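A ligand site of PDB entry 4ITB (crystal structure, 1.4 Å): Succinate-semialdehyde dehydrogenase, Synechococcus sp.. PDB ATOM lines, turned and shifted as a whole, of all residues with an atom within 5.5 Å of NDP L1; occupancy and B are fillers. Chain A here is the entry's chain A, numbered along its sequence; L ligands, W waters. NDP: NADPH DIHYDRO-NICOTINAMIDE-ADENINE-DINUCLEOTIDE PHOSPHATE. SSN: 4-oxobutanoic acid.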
ATOM      1  N   VAL A 129     -29.469 -23.717  18.173  1.00  0.00           N
ATOM      2  CA  VAL A 129     -28.880 -23.614  16.838  1.00  0.00           C
ATOM      3  C   VAL A 129     -27.367 -23.514  17.015  1.00  0.00           C
ATOM      4  O   VAL A 129     -26.863 -22.572  17.633  1.00  0.00           O
ATOM      5  CB  VAL A 129     -29.401 -22.371  16.089  1.00  0.00           C
ATOM      6  CG1 VAL A 129     -28.650 -22.209  14.774  1.00  0.00           C
ATOM      7  CG2 VAL A 129     -30.909 -22.499  15.847  1.00  0.00           C
ATOM      8  N   MET A 130     -26.652 -24.493  16.486  1.00  0.00           N
ATOM      9  CA  MET A 130     -25.237 -24.670  16.791  1.00  0.00           C
ATOM     10  C   MET A 130     -24.335 -24.625  15.562  1.00  0.00           C
ATOM     11  O   MET A 130     -24.775 -24.883  14.443  1.00  0.00           O
ATOM     12  CB  MET A 130     -25.037 -25.966  17.575  1.00  0.00           C
ATOM     13  CG  MET A 130     -25.682 -25.899  18.978  1.00  0.00           C
ATOM     14  SD  MET A 130     -24.825 -24.799  20.166  1.00  0.00           S
ATOM     15  CE  MET A 130     -26.143 -23.709  20.630  1.00  0.00           C
ATOM     16  N   PRO A 131     -23.060 -24.272  15.758  1.00  0.00           N
ATOM     17  CA  PRO A 131     -22.114 -24.138  14.647  1.00  0.00           C
ATOM     18  C   PRO A 131     -21.179 -25.339  14.492  1.00  0.00           C
ATOM     19  O   PRO A 131     -21.046 -26.171  15.385  1.00  0.00           O
ATOM     20  CB  PRO A 131     -21.307 -22.911  15.069  1.00  0.00           C
ATOM     21  CG  PRO A 131     -21.167 -23.132  16.539  1.00  0.00           C
ATOM     22  CD  PRO A 131     -22.498 -23.718  17.000  1.00  0.00           C
ATOM     23  N   TRP A 132     -20.498 -25.395  13.344  1.00  0.00           N
ATOM     24  CA  TRP A 132     -19.654 -26.537  13.007  1.00  0.00           C
ATOM     25  C   TRP A 132     -18.296 -26.536  13.706  1.00  0.00           C
ATOM     26  O   TRP A 132     -17.590 -27.539  13.628  1.00  0.00           O
ATOM     27  CB  TRP A 132     -19.435 -26.605  11.483  1.00  0.00           C
ATOM     28  CG  TRP A 132     -19.041 -25.270  10.920  1.00  0.00           C
ATOM     29  CD1 TRP A 132     -19.867 -24.380  10.293  1.00  0.00           C
ATOM     30  CD2 TRP A 132     -17.739 -24.650  10.969  1.00  0.00           C
ATOM     31  NE1 TRP A 132     -19.166 -23.243   9.954  1.00  0.00           N
ATOM     32  CE2 TRP A 132     -17.864 -23.383  10.359  1.00  0.00           C
ATOM     33  CE3 TRP A 132     -16.498 -25.048  11.470  1.00  0.00           C
ATOM     34  CZ2 TRP A 132     -16.783 -22.519  10.229  1.00  0.00           C
ATOM     35  CZ3 TRP A 132     -15.430 -24.168  11.350  1.00  0.00           C
ATOM     36  CH2 TRP A 132     -15.571 -22.926  10.728  1.00  0.00           C
ATOM     37  N   ASN A 133     -17.908 -25.440  14.356  1.00  0.00           N
ATOM     38  CA  ASN A 133     -16.501 -25.321  14.779  1.00  0.00           C
ATOM     39  C   ASN A 133     -16.135 -26.157  16.002  1.00  0.00           C
ATOM     40  O   ASN A 133     -15.004 -26.609  16.132  1.00  0.00           O
ATOM     41  CB  ASN A 133     -16.051 -23.866  14.905  1.00  0.00           C
ATOM     42  CG  ASN A 133     -16.751 -23.109  16.010  1.00  0.00           C
ATOM     43  OD1 ASN A 133     -17.903 -23.410  16.357  1.00  0.00           O
ATOM     44  ND2 ASN A 133     -16.060 -22.121  16.567  1.00  0.00           N
ATOM     45  N   GLN A 138     -19.987 -27.555  21.720  1.00  0.00           N
ATOM     46  CA  GLN A 138     -21.031 -26.536  21.768  1.00  0.00           C
ATOM     47  C   GLN A 138     -22.374 -27.147  22.104  1.00  0.00           C
ATOM     48  O   GLN A 138     -23.179 -26.569  22.846  1.00  0.00           O
ATOM     49  CB  GLN A 138     -21.151 -25.794  20.445  1.00  0.00           C
ATOM     50  CG  GLN A 138     -19.874 -25.151  19.977  1.00  0.00           C
ATOM     51  CD  GLN A 138     -19.827 -23.685  20.276  1.00  0.00           C
ATOM     52  OE1 GLN A 138     -20.464 -23.199  21.215  1.00  0.00           O
ATOM     53  NE2 GLN A 138     -19.081 -22.942  19.467  1.00  0.00           N
ATOM     54  N   LYS A 156     -30.766 -27.824  16.026  1.00  0.00           N
ATOM     55  CA  LYS A 156     -30.489 -27.569  14.613  1.00  0.00           C
ATOM     56  C   LYS A 156     -28.998 -27.299  14.523  1.00  0.00           C
ATOM     57  O   LYS A 156     -28.523 -26.234  14.920  1.00  0.00           O
ATOM     58  CB  LYS A 156     -31.318 -26.383  14.090  1.00  0.00           C
ATOM     59  CG  LYS A 156     -31.086 -26.078  12.597  1.00  0.00           C
ATOM     60  CD  LYS A 156     -30.083 -24.961  12.357  1.00  0.00           C
ATOM     61  CE  LYS A 156     -29.874 -24.700  10.850  1.00  0.00           C
ATOM     62  NZ  LYS A 156     -29.104 -25.785  10.180  1.00  0.00           N
ATOM     63  N   HIS A 157     -28.251 -28.300  14.075  1.00  0.00           N
ATOM     64  CA  HIS A 157     -26.819 -28.184  13.934  1.00  0.00           C
ATOM     65  C   HIS A 157     -26.489 -27.597  12.569  1.00  0.00           C
ATOM     66  O   HIS A 157     -27.359 -27.460  11.706  1.00  0.00           O
ATOM     67  CB  HIS A 157     -26.129 -29.536  14.110  1.00  0.00           C
ATOM     68  CG  HIS A 157     -24.837 -29.469  14.863  1.00  0.00           C
ATOM     69  ND1 HIS A 157     -24.007 -28.355  14.824  1.00  0.00           N
ATOM     70  CD2 HIS A 157     -24.235 -30.361  15.679  1.00  0.00           C
ATOM     71  CE1 HIS A 157     -22.952 -28.581  15.578  1.00  0.00           C
ATOM     72  NE2 HIS A 157     -23.061 -29.784  16.120  1.00  0.00           N
ATOM     73  N   ALA A 158     -25.222 -27.232  12.383  1.00  0.00           N
ATOM     74  CA  ALA A 158     -24.773 -26.726  11.104  1.00  0.00           C
ATOM     75  C   ALA A 158     -24.938 -27.795  10.030  1.00  0.00           C
ATOM     76  O   ALA A 158     -24.811 -29.002  10.290  1.00  0.00           O
ATOM     77  CB  ALA A 158     -23.329 -26.304  11.209  1.00  0.00           C
ATOM     78  N   SER A 159     -25.204 -27.351   8.804  1.00  0.00           N
ATOM     79  CA  SER A 159     -25.533 -28.260   7.706  1.00  0.00           C
ATOM     80  C   SER A 159     -24.367 -29.123   7.265  1.00  0.00           C
ATOM     81  O   SER A 159     -24.566 -30.132   6.576  1.00  0.00           O
ATOM     82  CB  SER A 159     -26.121 -27.497   6.517  1.00  0.00           C
ATOM     83  OG  SER A 159     -27.460 -27.129   6.767  1.00  0.00           O
ATOM     84  N   ASN A 160     -23.150 -28.734   7.649  1.00  0.00           N
ATOM     85  CA  ASN A 160     -21.950 -29.478   7.282  1.00  0.00           C
ATOM     86  C   ASN A 160     -21.461 -30.457   8.339  1.00  0.00           C
ATOM     87  O   ASN A 160     -20.456 -31.125   8.138  1.00  0.00           O
ATOM     88  CB  ASN A 160     -20.817 -28.509   6.895  1.00  0.00           C
ATOM     89  CG  ASN A 160     -20.497 -27.510   8.000  1.00  0.00           C
ATOM     90  OD1 ASN A 160     -21.396 -27.005   8.681  1.00  0.00           O
ATOM     91  ND2 ASN A 160     -19.216 -27.212   8.178  1.00  0.00           N
ATOM     92  N   ILE A 187     -32.177 -30.033   9.447  1.00  0.00           N
ATOM     93  CA  ILE A 187     -32.919 -28.985   8.752  1.00  0.00           C
ATOM     94  C   ILE A 187     -31.985 -27.840   8.425  1.00  0.00           C
ATOM     95  O   ILE A 187     -30.928 -27.671   9.055  1.00  0.00           O
ATOM     96  CB  ILE A 187     -34.110 -28.460   9.587  1.00  0.00           C
ATOM     97  CG1 ILE A 187     -33.627 -27.780  10.883  1.00  0.00           C
ATOM     98  CG2 ILE A 187     -35.075 -29.589   9.887  1.00  0.00           C
ATOM     99  CD1 ILE A 187     -34.754 -27.184  11.723  1.00  0.00           C
ATOM    100  N   GLY A 188     -32.363 -27.065   7.412  1.00  0.00           N
ATOM    101  CA  GLY A 188     -31.583 -25.911   7.003  1.00  0.00           C
ATOM    102  C   GLY A 188     -31.965 -24.651   7.757  1.00  0.00           C
ATOM    103  O   GLY A 188     -32.940 -24.613   8.516  1.00  0.00           O
ATOM    104  N   ALA A 189     -31.199 -23.596   7.515  1.00  0.00           N
ATOM    105  CA  ALA A 189     -31.423 -22.327   8.175  1.00  0.00           C
ATOM    106  C   ALA A 189     -32.828 -21.759   7.952  1.00  0.00           C
ATOM    107  O   ALA A 189     -33.415 -21.183   8.875  1.00  0.00           O
ATOM    108  CB  ALA A 189     -30.362 -21.313   7.751  1.00  0.00           C
ATOM    109  N   VAL A 192     -35.710 -22.916  10.483  1.00  0.00           N
ATOM    110  CA  VAL A 192     -35.667 -22.609  11.905  1.00  0.00           C
ATOM    111  C   VAL A 192     -36.850 -21.739  12.355  1.00  0.00           C
ATOM    112  O   VAL A 192     -37.363 -21.883  13.470  1.00  0.00           O
ATOM    113  CB  VAL A 192     -34.321 -21.965  12.264  1.00  0.00           C
ATOM    114  CG1 VAL A 192     -34.331 -21.462  13.694  1.00  0.00           C
ATOM    115  CG2 VAL A 192     -33.202 -22.979  12.077  1.00  0.00           C
ATOM    116  N   LEU A 206     -28.426 -19.612  20.329  1.00  0.00           N
ATOM    117  CA  LEU A 206     -27.633 -19.751  19.114  1.00  0.00           C
ATOM    118  C   LEU A 206     -26.190 -19.367  19.364  1.00  0.00           C
ATOM    119  O   LEU A 206     -25.906 -18.345  20.001  1.00  0.00           O
ATOM    120  CB  LEU A 206     -28.218 -18.877  17.988  1.00  0.00           C
ATOM    121  CG  LEU A 206     -27.534 -19.008  16.619  1.00  0.00           C
ATOM    122  CD1 LEU A 206     -28.535 -18.796  15.484  1.00  0.00           C
ATOM    123  CD2 LEU A 206     -26.371 -17.999  16.452  1.00  0.00           C
ATOM    124  N   THR A 207     -25.285 -20.198  18.846  1.00  0.00           N
ATOM    125  CA  THR A 207     -23.869 -19.853  18.762  1.00  0.00           C
ATOM    126  C   THR A 207     -23.499 -19.860  17.284  1.00  0.00           C
ATOM    127  O   THR A 207     -23.871 -20.789  16.541  1.00  0.00           O
ATOM    128  CB  THR A 207     -22.990 -20.837  19.543  1.00  0.00           C
ATOM    129  OG1 THR A 207     -23.319 -20.740  20.941  1.00  0.00           O
ATOM    130  CG2 THR A 207     -21.509 -20.518  19.349  1.00  0.00           C
ATOM    131  N   GLY A 208     -22.803 -18.827  16.819  1.00  0.00           N
ATOM    132  CA  GLY A 208     -22.497 -18.684  15.407  1.00  0.00           C
ATOM    133  C   GLY A 208     -22.243 -17.249  14.984  1.00  0.00           C
ATOM    134  O   GLY A 208     -21.712 -16.457  15.770  1.00  0.00           O
ATOM    135  N   SER A 209     -22.639 -16.914  13.767  1.00  0.00           N
ATOM    136  CA  SER A 209     -22.411 -15.582  13.181  1.00  0.00           C
ATOM    137  C   SER A 209     -23.457 -14.586  13.645  1.00  0.00           C
ATOM    138  O   SER A 209     -24.559 -14.959  14.052  1.00  0.00           O
ATOM    139  CB  SER A 209     -22.474 -15.639  11.648  1.00  0.00           C
ATOM    140  OG  SER A 209     -23.820 -15.823  11.182  1.00  0.00           O
ATOM    141  N   GLU A 210     -23.116 -13.311  13.542  1.00  0.00           N
ATOM    142  CA  GLU A 210     -24.078 -12.272  13.885  1.00  0.00           C
ATOM    143  C   GLU A 210     -25.366 -12.300  13.063  1.00  0.00           C
ATOM    144  O   GLU A 210     -26.440 -12.144  13.627  1.00  0.00           O
ATOM    145  CB  GLU A 210     -23.454 -10.865  13.874  1.00  0.00           C
ATOM    146  CG  GLU A 210     -24.442  -9.821  14.373  1.00  0.00           C
ATOM    147  CD  GLU A 210     -23.889  -8.426  14.442  1.00  0.00           C
ATOM    148  OE1 GLU A 210     -22.662  -8.290  14.608  1.00  0.00           O
ATOM    149  OE2 GLU A 210     -24.688  -7.471  14.321  1.00  0.00           O
ATOM    150  N   PRO A 211     -25.276 -12.487  11.722  1.00  0.00           N
ATOM    151  CA  PRO A 211     -26.549 -12.497  10.988  1.00  0.00           C
ATOM    152  C   PRO A 211     -27.491 -13.630  11.433  1.00  0.00           C
ATOM    153  O   PRO A 211     -28.702 -13.418  11.512  1.00  0.00           O
ATOM    154  CB  PRO A 211     -26.121 -12.675   9.540  1.00  0.00           C
ATOM    155  CG  PRO A 211     -24.747 -12.074   9.488  1.00  0.00           C
ATOM    156  CD  PRO A 211     -24.124 -12.473  10.808  1.00  0.00           C
ATOM    157  N   ALA A 212     -26.941 -14.802  11.714  1.00  0.00           N
ATOM    158  CA  ALA A 212     -27.736 -15.906  12.220  1.00  0.00           C
ATOM    159  C   ALA A 212     -28.353 -15.540  13.573  1.00  0.00           C
ATOM    160  O   ALA A 212     -29.556 -15.718  13.796  1.00  0.00           O
ATOM    161  CB  ALA A 212     -26.888 -17.165  12.337  1.00  0.00           C
ATOM    162  N   SER A 215     -31.196 -13.001  13.217  1.00  0.00           N
ATOM    163  CA  SER A 215     -32.397 -13.622  12.685  1.00  0.00           C
ATOM    164  C   SER A 215     -33.149 -14.382  13.779  1.00  0.00           C
ATOM    165  O   SER A 215     -34.352 -14.187  13.983  1.00  0.00           O
ATOM    166  CB  SER A 215     -32.020 -14.588  11.559  1.00  0.00           C
ATOM    167  OG  SER A 215     -33.179 -15.215  11.020  1.00  0.00           O
ATOM    168  N   LEU A 216     -32.432 -15.226  14.507  1.00  0.00           N
ATOM    169  CA  LEU A 216     -33.062 -16.012  15.557  1.00  0.00           C
ATOM    170  C   LEU A 216     -33.606 -15.138  16.678  1.00  0.00           C
ATOM    171  O   LEU A 216     -34.730 -15.344  17.151  1.00  0.00           O
ATOM    172  CB  LEU A 216     -32.094 -17.064  16.118  1.00  0.00           C
ATOM    173  CG  LEU A 216     -32.621 -17.918  17.286  1.00  0.00           C
ATOM    174  CD1 LEU A 216     -32.252 -19.387  17.091  1.00  0.00           C
ATOM    175  CD2 LEU A 216     -32.094 -17.416  18.638  1.00  0.00           C
ATOM    176  N   GLU A 230     -24.200 -16.395  21.601  1.00  0.00           N
ATOM    177  CA  GLU A 230     -22.751 -16.261  21.624  1.00  0.00           C
ATOM    178  C   GLU A 230     -22.278 -16.186  20.194  1.00  0.00           C
ATOM    179  O   GLU A 230     -22.331 -17.175  19.453  1.00  0.00           O
ATOM    180  CB  GLU A 230     -22.079 -17.404  22.364  1.00  0.00           C
ATOM    181  CG  GLU A 230     -20.583 -17.180  22.582  1.00  0.00           C
ATOM    182  CD  GLU A 230     -19.736 -18.005  21.633  1.00  0.00           C
ATOM    183  OE1 GLU A 230     -19.218 -17.431  20.657  1.00  0.00           O
ATOM    184  OE2 GLU A 230     -19.580 -19.213  21.881  1.00  0.00           O
ATOM    185  N   LEU A 231     -21.839 -15.008  19.793  1.00  0.00           N
ATOM    186  CA  LEU A 231     -21.470 -14.786  18.423  1.00  0.00           C
ATOM    187  C   LEU A 231     -19.937 -14.700  18.366  1.00  0.00           C
ATOM    188  O   LEU A 231     -19.256 -15.198  19.259  1.00  0.00           O
ATOM    189  CB  LEU A 231     -22.237 -13.570  17.885  1.00  0.00           C
ATOM    190  CG  LEU A 231     -23.743 -13.675  18.225  1.00  0.00           C
ATOM    191  CD1 LEU A 231     -24.514 -12.426  17.797  1.00  0.00           C
ATOM    192  CD2 LEU A 231     -24.408 -14.946  17.646  1.00  0.00           C
ATOM    193  N   GLY A 232     -19.395 -14.108  17.330  1.00  0.00           N
ATOM    194  CA  GLY A 232     -17.944 -14.114  17.224  1.00  0.00           C
ATOM    195  C   GLY A 232     -17.238 -13.176  18.183  1.00  0.00           C
ATOM    196  O   GLY A 232     -17.836 -12.548  19.068  1.00  0.00           O
ATOM    197  N   SER A 263     -12.113 -20.214  16.121  1.00  0.00           N
ATOM    198  CA  SER A 263     -12.681 -20.108  17.461  1.00  0.00           C
ATOM    199  C   SER A 263     -13.091 -18.686  17.749  1.00  0.00           C
ATOM    200  O   SER A 263     -12.380 -17.742  17.431  1.00  0.00           O
ATOM    201  CB  SER A 263     -11.684 -20.550  18.522  1.00  0.00           C
ATOM    202  OG  SER A 263     -12.206 -20.262  19.817  1.00  0.00           O
ATOM    203  N   CYS A 264     -14.256 -18.555  18.387  1.00  0.00           N
ATOM    204  CA  CYS A 264     -14.782 -17.288  18.843  1.00  0.00           C
ATOM    205  C   CYS A 264     -13.809 -16.560  19.784  1.00  0.00           C
ATOM    206  O   CYS A 264     -13.770 -15.344  19.805  1.00  0.00           O
ATOM    207  CB  CYS A 264     -16.121 -17.526  19.548  1.00  0.00           C
ATOM    208  SG  CYS A 264     -16.000 -18.561  21.044  1.00  0.00           S
ATOM    209  N   ILE A 311     -15.613 -20.436   4.000  1.00  0.00           N
ATOM    210  CA  ILE A 311     -14.708 -19.871   4.999  1.00  0.00           C
ATOM    211  C   ILE A 311     -13.358 -19.535   4.362  1.00  0.00           C
ATOM    212  O   ILE A 311     -12.779 -18.465   4.608  1.00  0.00           O
ATOM    213  CB  ILE A 311     -14.506 -20.840   6.183  1.00  0.00           C
ATOM    214  CG1 ILE A 311     -15.822 -21.080   6.911  1.00  0.00           C
ATOM    215  CG2 ILE A 311     -13.442 -20.294   7.136  1.00  0.00           C
ATOM    216  CD1 ILE A 311     -16.412 -19.838   7.541  1.00  0.00           C
ATOM    217  N   ASP A 314     -13.804 -16.466   2.202  1.00  0.00           N
ATOM    218  CA  ASP A 314     -13.957 -15.280   3.045  1.00  0.00           C
ATOM    219  C   ASP A 314     -12.614 -14.749   3.552  1.00  0.00           C
ATOM    220  O   ASP A 314     -12.308 -13.572   3.381  1.00  0.00           O
ATOM    221  CB  ASP A 314     -14.893 -15.567   4.221  1.00  0.00           C
ATOM    222  CG  ASP A 314     -16.352 -15.717   3.787  1.00  0.00           C
ATOM    223  OD1 ASP A 314     -16.710 -15.289   2.670  1.00  0.00           O
ATOM    224  OD2 ASP A 314     -17.133 -16.270   4.595  1.00  0.00           O
ATOM    225  N   GLU A 361     -14.128 -10.233  12.018  1.00  0.00           N
ATOM    226  CA  GLU A 361     -13.620 -11.447  12.648  1.00  0.00           C
ATOM    227  C   GLU A 361     -12.875 -12.298  11.632  1.00  0.00           C
ATOM    228  O   GLU A 361     -13.411 -12.642  10.571  1.00  0.00           O
ATOM    229  CB  GLU A 361     -14.749 -12.289  13.257  1.00  0.00           C
ATOM    230  CG  GLU A 361     -14.233 -13.574  13.909  1.00  0.00           C
ATOM    231  CD  GLU A 361     -15.289 -14.336  14.701  1.00  0.00           C
ATOM    232  OE1 GLU A 361     -16.442 -14.447  14.213  1.00  0.00           O
ATOM    233  OE2 GLU A 361     -14.964 -14.856  15.794  1.00  0.00           O
ATOM    234  N   PHE A 363     -11.630 -15.720  10.896  1.00  0.00           N
ATOM    235  CA  PHE A 363     -11.940 -17.069  11.355  1.00  0.00           C
ATOM    236  C   PHE A 363     -11.044 -18.048  10.621  1.00  0.00           C
ATOM    237  O   PHE A 363     -11.495 -18.846   9.790  1.00  0.00           O
ATOM    238  CB  PHE A 363     -13.426 -17.393  11.116  1.00  0.00           C
ATOM    239  CG  PHE A 363     -14.101 -18.095  12.274  1.00  0.00           C
ATOM    240  CD1 PHE A 363     -14.142 -17.516  13.538  1.00  0.00           C
ATOM    241  CD2 PHE A 363     -14.714 -19.331  12.084  1.00  0.00           C
ATOM    242  CE1 PHE A 363     -14.775 -18.159  14.595  1.00  0.00           C
ATOM    243  CE2 PHE A 363     -15.347 -19.986  13.150  1.00  0.00           C
ATOM    244  CZ  PHE A 363     -15.376 -19.390  14.402  1.00  0.00           C
HETATM  245  PA  NDP L   1     -23.497 -19.374  10.629  1.00  0.00           P
HETATM  246  O1A NDP L   1     -23.833 -18.339  11.668  1.00  0.00           O
HETATM  247  O2A NDP L   1     -24.152 -19.276   9.282  1.00  0.00           O
HETATM  248  O5B NDP L   1     -23.929 -20.817  11.220  1.00  0.00           O
HETATM  249  C5B NDP L   1     -24.183 -21.088  12.598  1.00  0.00           C
HETATM  250  C4B NDP L   1     -25.492 -21.870  12.751  1.00  0.00           C
HETATM  251  O4B NDP L   1     -26.591 -20.990  12.483  1.00  0.00           O
HETATM  252  C3B NDP L   1     -25.650 -23.029  11.783  1.00  0.00           C
HETATM  253  O3B NDP L   1     -26.441 -24.049  12.400  1.00  0.00           O
HETATM  254  C2B NDP L   1     -26.445 -22.382  10.665  1.00  0.00           C
HETATM  255  O2B NDP L   1     -27.159 -23.326   9.886  1.00  0.00           O
HETATM  256  C1B NDP L   1     -27.401 -21.560  11.468  1.00  0.00           C
HETATM  257  N9A NDP L   1     -28.002 -20.420  10.776  1.00  0.00           N
HETATM  258  C8A NDP L   1     -27.436 -19.620   9.844  1.00  0.00           C
HETATM  259  N7A NDP L   1     -28.302 -18.643   9.477  1.00  0.00           N
HETATM  260  C5A NDP L   1     -29.427 -18.811  10.205  1.00  0.00           C
HETATM  261  C6A NDP L   1     -30.728 -18.160  10.319  1.00  0.00           C
HETATM  262  N6A NDP L   1     -31.022 -17.068   9.572  1.00  0.00           N
HETATM  263  N1A NDP L   1     -31.601 -18.683  11.205  1.00  0.00           N
HETATM  264  C2A NDP L   1     -31.336 -19.762  11.957  1.00  0.00           C
HETATM  265  N3A NDP L   1     -30.177 -20.412  11.888  1.00  0.00           N
HETATM  266  C4A NDP L   1     -29.212 -19.989  11.049  1.00  0.00           C
HETATM  267  O3  NDP L   1     -21.903 -19.451  10.414  1.00  0.00           O
HETATM  268  PN  NDP L   1     -21.054 -19.685   9.051  1.00  0.00           P
HETATM  269  O1N NDP L   1     -21.669 -19.008   7.849  1.00  0.00           O
HETATM  270  O2N NDP L   1     -20.697 -21.150   8.971  1.00  0.00           O
HETATM  271  O5D NDP L   1     -19.731 -18.887   9.484  1.00  0.00           O
HETATM  272  C5D NDP L   1     -19.629 -17.504   9.127  1.00  0.00           C
HETATM  273  C4D NDP L   1     -18.892 -16.725  10.219  1.00  0.00           C
HETATM  274  O4D NDP L   1     -19.647 -16.700  11.431  1.00  0.00           O
HETATM  275  C3D NDP L   1     -17.567 -17.354  10.612  1.00  0.00           C
HETATM  276  O3D NDP L   1     -16.513 -16.965   9.740  1.00  0.00           O
HETATM  277  C2D NDP L   1     -17.370 -16.791  11.988  1.00  0.00           C
HETATM  278  O2D NDP L   1     -16.914 -15.431  11.863  1.00  0.00           O
HETATM  279  C1D NDP L   1     -18.783 -16.789  12.576  1.00  0.00           C
HETATM  280  N1N NDP L   1     -19.014 -18.022  13.369  1.00  0.00           N
HETATM  281  C2N NDP L   1     -18.938 -17.949  14.702  1.00  0.00           C
HETATM  282  C3N NDP L   1     -18.843 -19.092  15.491  1.00  0.00           C
HETATM  283  C7N NDP L   1     -18.770 -18.991  16.987  1.00  0.00           C
HETATM  284  O7N NDP L   1     -18.251 -19.884  17.635  1.00  0.00           O
HETATM  285  N7N NDP L   1     -19.286 -17.931  17.594  1.00  0.00           N
HETATM  286  C4N NDP L   1     -18.816 -20.466  14.867  1.00  0.00           C
HETATM  287  C5N NDP L   1     -19.199 -20.411  13.458  1.00  0.00           C
HETATM  288  C6N NDP L   1     -19.287 -19.207  12.782  1.00  0.00           C
HETATM  289  P2B NDP L   1     -26.629 -23.810   8.446  1.00  0.00           P
HETATM  290  O1X NDP L   1     -27.720 -24.727   8.000  1.00  0.00           O
HETATM  291  O2X NDP L   1     -26.551 -22.550   7.610  1.00  0.00           O
HETATM  292  O3X NDP L   1     -25.298 -24.462   8.630  1.00  0.00           O
HETATM  293  C1  SSN L   2     -14.893 -22.442  23.153  1.00  0.00           C
HETATM  294  O1  SSN L   2     -15.759 -22.619  24.054  1.00  0.00           O
HETATM  295  C2  SSN L   2     -15.163 -21.585  21.965  1.00  0.00           C
HETATM  296  O2  SSN L   2     -13.771 -22.986  23.261  1.00  0.00           O
HETATM  297  C3  SSN L   2     -16.544 -21.127  21.658  1.00  0.00           C
HETATM  298  C4  SSN L   2     -16.738 -20.217  20.488  1.00  0.00           C
HETATM  299  O4  SSN L   2     -16.180 -20.574  19.271  1.00  0.00           O
HETATM  300  O   HOH W   1     -22.971 -25.038   6.826  1.00  0.00           O
HETATM  301  O   HOH W   2     -21.781 -22.896  11.776  1.00  0.00           O
HETATM  302  O   HOH W   3     -22.837 -23.350   9.248  1.00  0.00           O
HETATM  303  O   HOH W   4     -34.315 -18.006  11.393  1.00  0.00           O
HETATM  304  O   HOH W   5     -29.032 -23.935   5.661  1.00  0.00           O
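OG of Ser 215 is in hydrogen-bond range of N6A of NDP L1. An oxygen (O4) of SSN L2 lies within hydrogen-bond range of the side-chain amide nitrogen (ND2) of Asn 133 (3.1 Å). OG of Ser 209 sits at hydrogen-bond distance from O1A of NDP L1, 2.6 Å away. O7N of NDP L1 is in hydrogen-bond range of ND2 of Asn 133, 3.3 Å away. N of Ser 209 is in hydrogen-bond range of O1A of NDP L1, at 2.8 Å. The side-chain amino group of Lys 156 lies within salt-bridge range of an oxygen (O1X) of NDP L1 (2.8 Å). The side-chain hydroxyl of Ser 159 lies within hydrogen-bond range of an oxygen (O1X) of NDP L1 (2.7 Å). OE1 of Glu 230 sits at hydrogen-bond distance from N7N of NDP L1 (3.1 Å). The side-chain carboxylate (OE1) of Glu 361 is in hydrogen-bond range of an oxygen (O2D) of NDP L1, 2.6 Å away. N7N of NDP L1 is in hydrogen-bond range of O of Leu 231 (3.2 Å). The backbone carbonyl oxygen (O) of Met 130 is in hydrogen-bond range of an oxygen (O3B) of NDP L1, 2.8 Å away. N of Ser 159 lies within hydrogen-bond range of O3X of NDP L1, at 2.9 Å. The backbone NH of Cys 264 sits at hydrogen-bond distance from an oxygen (O4) of SSN L2 (2.9 Å). The backbone NH of Ala 158 sits at hydrogen-bond distance from an oxygen (O3B) of NDP L1 (3.4 Å). NE1 of Trp 132 is in hydrogen-bond range of O2N of NDP L1, at 2.8 Å. The side-chain sulfur (SG) of Cys 264 is covalently linked to a carbon (C4) of SSN L2. A nitrogen (N7N) of NDP L1 lies close to the backbone carbonyl oxygen (O) of Gly 208, at 3.4 Å.
An oxygen (O4) of SSN L2 lies close to an oxygen (O7N) of NDP L1, 2.7 Å away.
The backbone NH of Glu 230 lies within hydrogen-bond range of the backbone carbonyl oxygen of Leu 206, 3.0 Å away. NZ of Lys 156 is in hydrogen-bond range of O of Ile 187 (2.9 Å). OG of Ser 209 lies within hydrogen-bond range of N of Ala 212, at 3.3 Å. The side-chain amide oxygen (OD1) of Asn 133 sits at hydrogen-bond distance from the side-chain amide nitrogen (NE2) of Gln 138 (3.4 Å). The backbone carbonyl oxygen (O) of Glu 230 sits at hydrogen-bond distance from the backbone NH (N) of Gly 208 (3.1 Å). The backbone NH (N) of Thr 207 is in hydrogen-bond range of the backbone carbonyl oxygen (O) of Val 129 (3.1 Å). The backbone NH (N) of Ala 158 is in hydrogen-bond range of the backbone carbonyl oxygen (O) of Met 130 (3.2 Å). The backbone NH of Met 130 sits at hydrogen-bond distance from the backbone carbonyl oxygen of Lys 156, 3.0 Å away.
Val 129 touches NDP L1 (CG1 to O4B, 3.3 Å). Pro 131 touches NDP L1 (CB to C4N, 3.5 Å). Gln 138 touches NDP L1. C of His 157 touches O3B of NDP L1, at 3.6 Å. Ala 189 touches NDP L1. CG2 of Val 192 touches C2A of NDP L1, 3.7 Å away. Thr 207 touches NDP L1 (CG2 to O7N, 3.7 Å). Ala 212 touches NDP L1. Gly 232 touches NDP L1 (N to N7N, 3.8 Å). Cys 264 touches NDP L1. CD1 of Ile 311 touches O3D of NDP L1, at 3.6 Å. Phe 363 touches NDP L1 (CB to O3D, 3.4 Å). Hydrophobic or aromatic side chains that line NDP L1: Val 129, Pro 131, Trp 132, Ala 158, Ala 189, Val 192, Ala 212, Ile 311 and Phe 363. Within 4 Å of NDP L1: Val 129, Met 130, Pro 131, Trp 132, Asn 133, Gln 138, Lys 156, His 157, Ala 158, Ser 159, Ala 189, Val 192, Thr 207, Gly 208, Ser 209, Ala 212, Ser 215, Glu 230, Leu 231, Gly 232, Cys 264, Ile 311, Glu 361 and Phe 363.
Water W5 bridges O1X of NDP L1 (2.8 Å) and N of Ala 189 (2.9 Å). Water W4 lies within hydrogen-bond range of N1A of NDP L1 (2.8 Å) and OG of Ser 215 (3.0 Å). Water W1 lies within hydrogen-bond range of an oxygen (O3X) of NDP L1 (3.0 Å) and the side-chain amide oxygen of Asn 160 (3.1 Å). Water W2 bridges an oxygen (O5B) of NDP L1 and the indole nitrogen of Trp 132.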
